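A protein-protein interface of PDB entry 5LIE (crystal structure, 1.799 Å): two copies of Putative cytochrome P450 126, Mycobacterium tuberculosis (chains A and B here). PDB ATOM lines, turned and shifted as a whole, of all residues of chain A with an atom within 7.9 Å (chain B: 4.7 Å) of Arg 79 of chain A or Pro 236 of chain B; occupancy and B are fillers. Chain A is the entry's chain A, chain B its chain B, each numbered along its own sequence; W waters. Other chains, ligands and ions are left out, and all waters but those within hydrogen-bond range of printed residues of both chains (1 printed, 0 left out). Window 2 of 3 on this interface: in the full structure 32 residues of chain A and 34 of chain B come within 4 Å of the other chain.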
ATOM      1  N   VAL A  73     -24.411  -4.283 -21.501  1.00  0.00           N
ATOM      2  CA  VAL A  73     -23.480  -3.787 -22.485  1.00  0.00           C
ATOM      3  C   VAL A  73     -23.667  -2.285 -22.657  1.00  0.00           C
ATOM      4  O   VAL A  73     -22.809  -1.515 -22.265  1.00  0.00           O
ATOM      5  CB  VAL A  73     -23.651  -4.456 -23.860  1.00  0.00           C
ATOM      6  CG1 VAL A  73     -22.600  -3.898 -24.853  1.00  0.00           C
ATOM      7  CG2 VAL A  73     -23.501  -5.974 -23.744  1.00  0.00           C
ATOM      8  N   THR A  74     -24.814  -1.872 -23.201  1.00  0.00           N
ATOM      9  CA  THR A  74     -25.059  -0.447 -23.431  1.00  0.00           C
ATOM     10  C   THR A  74     -26.522  -0.246 -23.851  1.00  0.00           C
ATOM     11  O   THR A  74     -27.286  -1.211 -23.897  1.00  0.00           O
ATOM     12  CB  THR A  74     -24.084   0.156 -24.492  1.00  0.00           C
ATOM     13  OG1 THR A  74     -24.059   1.588 -24.360  1.00  0.00           O
ATOM     14  CG2 THR A  74     -24.504  -0.200 -25.911  1.00  0.00           C
ATOM     15  N   GLY A  75     -26.910   0.976 -24.187  1.00  0.00           N
ATOM     16  CA  GLY A  75     -28.250   1.201 -24.724  1.00  0.00           C
ATOM     17  C   GLY A  75     -28.428   2.623 -25.221  1.00  0.00           C
ATOM     18  O   GLY A  75     -27.592   3.462 -24.954  1.00  0.00           O
ATOM     19  N   GLY A  76     -29.528   2.901 -25.921  1.00  0.00           N
ATOM     20  CA  GLY A  76     -29.725   4.255 -26.423  1.00  0.00           C
ATOM     21  C   GLY A  76     -28.557   4.685 -27.308  1.00  0.00           C
ATOM     22  O   GLY A  76     -28.070   3.901 -28.117  1.00  0.00           O
ATOM     23  N   GLN A  77     -28.105   5.928 -27.145  1.00  0.00           N
ATOM     24  CA  GLN A  77     -27.012   6.449 -27.959  1.00  0.00           C
ATOM     25  C   GLN A  77     -25.663   6.275 -27.284  1.00  0.00           C
ATOM     26  O   GLN A  77     -24.646   6.732 -27.804  1.00  0.00           O
ATOM     27  CB  GLN A  77     -27.243   7.931 -28.249  1.00  0.00           C
ATOM     28  CG  GLN A  77     -28.599   8.200 -28.907  1.00  0.00           C
ATOM     29  CD  GLN A  77     -28.764   7.406 -30.182  1.00  0.00           C
ATOM     30  OE1 GLN A  77     -29.635   6.541 -30.290  1.00  0.00           O
ATOM     31  NE2 GLN A  77     -27.898   7.685 -31.165  1.00  0.00           N
ATOM     32  N   ARG A  78     -25.640   5.577 -26.148  1.00  0.00           N
ATOM     33  CA  ARG A  78     -24.410   5.428 -25.391  1.00  0.00           C
ATOM     34  C   ARG A  78     -23.456   4.451 -26.085  1.00  0.00           C
ATOM     35  O   ARG A  78     -23.875   3.363 -26.460  1.00  0.00           O
ATOM     36  CB  ARG A  78     -24.756   4.952 -23.957  1.00  0.00           C
ATOM     37  CG  ARG A  78     -23.513   4.865 -23.029  1.00  0.00           C
ATOM     38  CD  ARG A  78     -23.915   4.361 -21.616  1.00  0.00           C
ATOM     39  NE  ARG A  78     -24.908   5.206 -20.971  1.00  0.00           N
ATOM     40  CZ  ARG A  78     -24.621   6.356 -20.381  1.00  0.00           C
ATOM     41  NH1 ARG A  78     -23.353   6.798 -20.331  1.00  0.00           N
ATOM     42  NH2 ARG A  78     -25.590   7.080 -19.840  1.00  0.00           N
ATOM     43  N   ARG A  79     -22.188   4.823 -26.295  1.00  0.00           N
ATOM     44  CA  ARG A  79     -21.330   3.962 -27.111  1.00  0.00           C
ATOM     45  C   ARG A  79     -20.905   2.690 -26.346  1.00  0.00           C
ATOM     46  O   ARG A  79     -20.902   1.610 -26.902  1.00  0.00           O
ATOM     47  CB  ARG A  79     -20.093   4.738 -27.588  1.00  0.00           C
ATOM     48  CG  ARG A  79     -20.499   5.893 -28.574  1.00  0.00           C
ATOM     49  CD  ARG A  79     -19.450   6.996 -28.625  1.00  0.00           C
ATOM     50  NE  ARG A  79     -18.166   6.390 -28.784  1.00  0.00           N
ATOM     51  CZ  ARG A  79     -17.062   6.817 -28.197  1.00  0.00           C
ATOM     52  NH1 ARG A  79     -17.064   7.899 -27.414  1.00  0.00           N
ATOM     53  NH2 ARG A  79     -15.952   6.148 -28.418  1.00  0.00           N
ATOM     54  N   PHE A  80     -20.561   2.830 -25.083  1.00  0.00           N
ATOM     55  CA  PHE A  80     -20.242   1.632 -24.271  1.00  0.00           C
ATOM     56  C   PHE A  80     -20.664   1.847 -22.822  1.00  0.00           C
ATOM     57  O   PHE A  80     -20.702   2.988 -22.337  1.00  0.00           O
ATOM     58  CB  PHE A  80     -18.762   1.247 -24.381  1.00  0.00           C
ATOM     59  CG  PHE A  80     -17.828   2.402 -24.376  1.00  0.00           C
ATOM     60  CD1 PHE A  80     -17.457   3.012 -23.172  1.00  0.00           C
ATOM     61  CD2 PHE A  80     -17.296   2.881 -25.571  1.00  0.00           C
ATOM     62  CE1 PHE A  80     -16.566   4.129 -23.143  1.00  0.00           C
ATOM     63  CE2 PHE A  80     -16.404   3.981 -25.573  1.00  0.00           C
ATOM     64  CZ  PHE A  80     -16.031   4.603 -24.357  1.00  0.00           C
ATOM     65  N   GLY A  81     -20.956   0.756 -22.108  1.00  0.00           N
ATOM     66  CA  GLY A  81     -21.510   0.869 -20.790  1.00  0.00           C
ATOM     67  C   GLY A  81     -20.809  -0.178 -19.924  1.00  0.00           C
ATOM     68  O   GLY A  81     -19.690   0.067 -19.478  1.00  0.00           O
ATOM     69  N   GLY A  82     -21.441  -1.343 -19.764  1.00  0.00           N
ATOM     70  CA  GLY A  82     -20.912  -2.414 -18.917  1.00  0.00           C
ATOM     71  C   GLY A  82     -21.701  -2.519 -17.622  1.00  0.00           C
ATOM     72  O   GLY A  82     -22.876  -2.142 -17.564  1.00  0.00           O
ATOM     73  N   ASP A  87     -18.563   4.024 -17.555  1.00  0.00           N
ATOM     74  CA  ASP A  87     -18.587   3.341 -18.873  1.00  0.00           C
ATOM     75  C   ASP A  87     -17.198   2.816 -19.202  1.00  0.00           C
ATOM     76  O   ASP A  87     -16.205   3.541 -19.009  1.00  0.00           O
ATOM     77  CB  ASP A  87     -18.942   4.311 -19.967  1.00  0.00           C
ATOM     78  CG  ASP A  87     -20.419   4.717 -19.953  1.00  0.00           C
ATOM     79  OD1 ASP A  87     -21.218   4.133 -19.190  1.00  0.00           O
ATOM     80  OD2 ASP A  87     -20.751   5.675 -20.711  1.00  0.00           O
ATOM     81  N   LEU A  88     -17.114   1.588 -19.688  1.00  0.00           N
ATOM     82  CA  LEU A  88     -15.821   0.969 -19.982  1.00  0.00           C
ATOM     83  C   LEU A  88     -15.826   0.479 -21.417  1.00  0.00           C
ATOM     84  O   LEU A  88     -16.796  -0.127 -21.861  1.00  0.00           O
ATOM     85  CB  LEU A  88     -15.584  -0.233 -19.031  1.00  0.00           C
ATOM     86  CG  LEU A  88     -15.297   0.090 -17.559  1.00  0.00           C
ATOM     87  CD1 LEU A  88     -15.262  -1.212 -16.749  1.00  0.00           C
ATOM     88  CD2 LEU A  88     -13.964   0.857 -17.405  1.00  0.00           C
ATOM     89  N   PRO A  89     -14.735   0.715 -22.154  1.00  0.00           N
ATOM     90  CA  PRO A  89     -14.653   0.203 -23.519  1.00  0.00           C
ATOM     91  C   PRO A  89     -14.598  -1.313 -23.600  1.00  0.00           C
ATOM     92  O   PRO A  89     -14.794  -1.824 -24.715  1.00  0.00           O
ATOM     93  CB  PRO A  89     -13.344   0.823 -24.065  1.00  0.00           C
ATOM     94  CG  PRO A  89     -13.014   1.950 -23.121  1.00  0.00           C
ATOM     95  CD  PRO A  89     -13.551   1.531 -21.789  1.00  0.00           C
ATOM     96  N   ALA A  91     -16.841  -3.146 -22.302  1.00  0.00           N
ATOM     97  CA  ALA A  91     -18.227  -3.596 -22.380  1.00  0.00           C
ATOM     98  C   ALA A  91     -18.458  -4.372 -23.666  1.00  0.00           C
ATOM     99  O   ALA A  91     -18.004  -3.951 -24.757  1.00  0.00           O
ATOM    100  CB  ALA A  91     -19.196  -2.384 -22.297  1.00  0.00           C
ATOM    101  N   GLN B  93     -10.727   3.893 -29.686  1.00  0.00           N
ATOM    102  CA  GLN B  93     -10.912   4.742 -28.516  1.00  0.00           C
ATOM    103  C   GLN B  93      -9.709   5.619 -28.191  1.00  0.00           C
ATOM    104  O   GLN B  93      -9.742   6.384 -27.228  1.00  0.00           O
ATOM    105  CB  GLN B  93     -11.191   3.873 -27.270  1.00  0.00           C
ATOM    106  CG  GLN B  93     -12.632   3.739 -26.945  1.00  0.00           C
ATOM    107  CD  GLN B  93     -13.293   2.748 -27.821  1.00  0.00           C
ATOM    108  OE1 GLN B  93     -13.075   1.535 -27.679  1.00  0.00           O
ATOM    109  NE2 GLN B  93     -14.103   3.234 -28.754  1.00  0.00           N
ATOM    110  N   ARG B 102     -13.480   9.941 -37.545  1.00  0.00           N
ATOM    111  CA  ARG B 102     -13.220  10.424 -36.205  1.00  0.00           C
ATOM    112  C   ARG B 102     -11.755  10.862 -36.036  1.00  0.00           C
ATOM    113  O   ARG B 102     -11.461  11.838 -35.349  1.00  0.00           O
ATOM    114  CB  ARG B 102     -13.621   9.398 -35.139  1.00  0.00           C
ATOM    115  CG  ARG B 102     -13.659  10.003 -33.736  1.00  0.00           C
ATOM    116  CD  ARG B 102     -13.887   8.920 -32.654  1.00  0.00           C
ATOM    117  NE  ARG B 102     -14.152   9.488 -31.325  1.00  0.00           N
ATOM    118  CZ  ARG B 102     -14.064   8.799 -30.191  1.00  0.00           C
ATOM    119  NH1 ARG B 102     -13.720   7.513 -30.217  1.00  0.00           N
ATOM    120  NH2 ARG B 102     -14.341   9.386 -29.023  1.00  0.00           N
ATOM    121  N   ILE B 106     -10.281  14.365 -34.110  1.00  0.00           N
ATOM    122  CA  ILE B 106      -9.504  14.327 -32.861  1.00  0.00           C
ATOM    123  C   ILE B 106      -8.052  14.718 -33.092  1.00  0.00           C
ATOM    124  O   ILE B 106      -7.452  15.322 -32.232  1.00  0.00           O
ATOM    125  CB  ILE B 106      -9.574  12.939 -32.180  1.00  0.00           C
ATOM    126  CG1 ILE B 106     -11.042  12.575 -31.977  1.00  0.00           C
ATOM    127  CG2 ILE B 106      -8.810  12.937 -30.858  1.00  0.00           C
ATOM    128  CD1 ILE B 106     -11.848  13.659 -31.251  1.00  0.00           C
ATOM    129  N   PRO B 236     -17.502  11.324 -32.360  1.00  0.00           N
ATOM    130  CA  PRO B 236     -17.759  11.715 -30.964  1.00  0.00           C
ATOM    131  C   PRO B 236     -16.547  12.350 -30.266  1.00  0.00           C
ATOM    132  O   PRO B 236     -15.387  12.024 -30.567  1.00  0.00           O
ATOM    133  CB  PRO B 236     -18.092  10.383 -30.275  1.00  0.00           C
ATOM    134  CG  PRO B 236     -18.295   9.369 -31.377  1.00  0.00           C
ATOM    135  CD  PRO B 236     -17.499   9.863 -32.544  1.00  0.00           C
ATOM    136  N   ALA B 237     -16.827  13.236 -29.317  1.00  0.00           N
ATOM    137  CA  ALA B 237     -15.794  13.802 -28.449  1.00  0.00           C
ATOM    138  C   ALA B 237     -15.279  12.705 -27.541  1.00  0.00           C
ATOM    139  O   ALA B 237     -15.866  11.615 -27.464  1.00  0.00           O
ATOM    140  CB  ALA B 237     -16.372  14.950 -27.601  1.00  0.00           C
ATOM    141  N   LEU B 238     -14.207  12.991 -26.827  1.00  0.00           N
ATOM    142  CA  LEU B 238     -13.608  11.962 -26.022  1.00  0.00           C
ATOM    143  C   LEU B 238     -14.452  11.804 -24.749  1.00  0.00           C
ATOM    144  O   LEU B 238     -14.667  12.757 -23.984  1.00  0.00           O
ATOM    145  CB  LEU B 238     -12.135  12.264 -25.706  1.00  0.00           C
ATOM    146  CG  LEU B 238     -11.165  12.317 -26.901  1.00  0.00           C
ATOM    147  CD1 LEU B 238      -9.735  12.307 -26.422  1.00  0.00           C
ATOM    148  CD2 LEU B 238     -11.355  11.146 -27.850  1.00  0.00           C
ATOM    149  N   SER B 239     -14.922  10.586 -24.534  1.00  0.00           N
ATOM    150  CA  SER B 239     -15.513  10.227 -23.262  1.00  0.00           C
ATOM    151  C   SER B 239     -14.419  10.245 -22.176  1.00  0.00           C
ATOM    152  O   SER B 239     -13.236  10.327 -22.479  1.00  0.00           O
ATOM    153  CB  SER B 239     -16.090   8.818 -23.387  1.00  0.00           C
ATOM    154  OG  SER B 239     -15.030   7.871 -23.457  1.00  0.00           O
ATOM    155  N   GLU B 242     -11.897   7.565 -22.619  1.00  0.00           N
ATOM    156  CA  GLU B 242     -10.991   7.944 -23.692  1.00  0.00           C
ATOM    157  C   GLU B 242     -10.010   9.037 -23.283  1.00  0.00           C
ATOM    158  O   GLU B 242      -8.867   9.056 -23.744  1.00  0.00           O
ATOM    159  CB  GLU B 242     -11.785   8.353 -24.911  1.00  0.00           C
ATOM    160  CG  GLU B 242     -12.619   7.161 -25.395  1.00  0.00           C
ATOM    161  CD  GLU B 242     -13.594   7.508 -26.463  1.00  0.00           C
ATOM    162  OE1 GLU B 242     -13.651   6.753 -27.451  1.00  0.00           O
ATOM    163  OE2 GLU B 242     -14.313   8.513 -26.319  1.00  0.00           O
HETATM  164  O   HOH W   1     -18.303  11.017 -26.654  1.00  0.00           O
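No position is printed for both chains.
Of the 8 pairs that touch across the chains among the printed residues, none has its exchanged pair printed and touching as well.
CD of Arg 79 of chain A touches CG of Pro 236 of chain B, at 3.8 Å.
NH1 of Arg 79 of chain A touches O of Ala 237 of chain B (3.9 Å).
Gln 93 of chain B touches Phe 80 of chain A.
Ser 239 of chain B touches Phe 80 of chain A.
OE1 of Gln 93 of chain B touches CB of Pro 89 of chain A (3.7 Å).
The guanidinium group of Arg 79 of chain A sits close to the side-chain amide nitrogen of Gln 93 of chain B, 3.5 Å away.
The side-chain carboxylate (OE1) of Glu 242 of chain B is in salt-bridge range of the guanidinium group (NH2) of Arg 79 of chain A (2.6 Å).
NH1 of Arg 102 of chain B sits close to NH2 of Arg 79 of chain A (3.2 Å).
Water W1 lies within hydrogen-bond range of O of Ala 237 of chain B and NH1 of Arg 79 of chain A.
Val 73 of chain A touches none of the printed residues of chain B.
Gly 76 of chain A touches none of the printed residues of chain B.
Of chain B, only Gln 93 (3.5 Å), Arg 102 (3.2 Å), Pro 236 (3.8 Å), Ala 237 (3.9 Å) and Glu 242 (2.6 Å) come within 4 Å of Arg 79 of chain A.
Of the printed residues of chain B, Phe 80 of chain A touches Gln 93 and Ser 239.
Of the printed residues of chain A, Gln 93 of chain B touches Arg 79, Phe 80 and Pro 89.
Printed residues of chain A within 4 Å of Arg 102 of chain B: Arg 79.
Pro 236 of chain B touches just one residue of chain A: Arg 79 (3.8 Å).
Of chain A, only Arg 79 comes within 4 Å of Ala 237 of chain B.
The nearest residue of chain A that does not touch Pro 236 of chain B is Gln 77 of chain A (7.7 Å).
O of Pro 236 of chain B is in hydrogen-bond range of NE of Arg 102 of chain B, 2.9 Å away.
The guanidinium group (NH2) of Arg 102 of chain B sits at hydrogen-bond distance from the backbone carbonyl oxygen (O) of Ala 237 of chain B (3.1 Å).
The side-chain carboxylate (OE2) of Glu 242 of chain B lies within salt-bridge range of the guanidinium group (NH2) of Arg 102 of chain B (2.8 Å).
N of Ser 239 of chain B sits at hydrogen-bond distance from OE2 of Glu 242 of chain B (2.8 Å).
Hydrophobic or aromatic side chains of chain A that line the printed part of chain B: Phe 80 and Pro 89.
Of the 8 printed residues of chain B, 6 touch a printed residue of chain A.
Hydrophobic or aromatic side chains of chain B within 4 Å of the printed part of chain A: Pro 236.
Among the printed residues, Asp or Glu carboxylates within 4 Å of a Lys or Arg side-chain nitrogen of the other chain: Arg 79 of chain A with Glu 242 of chain B (2.6 Å).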
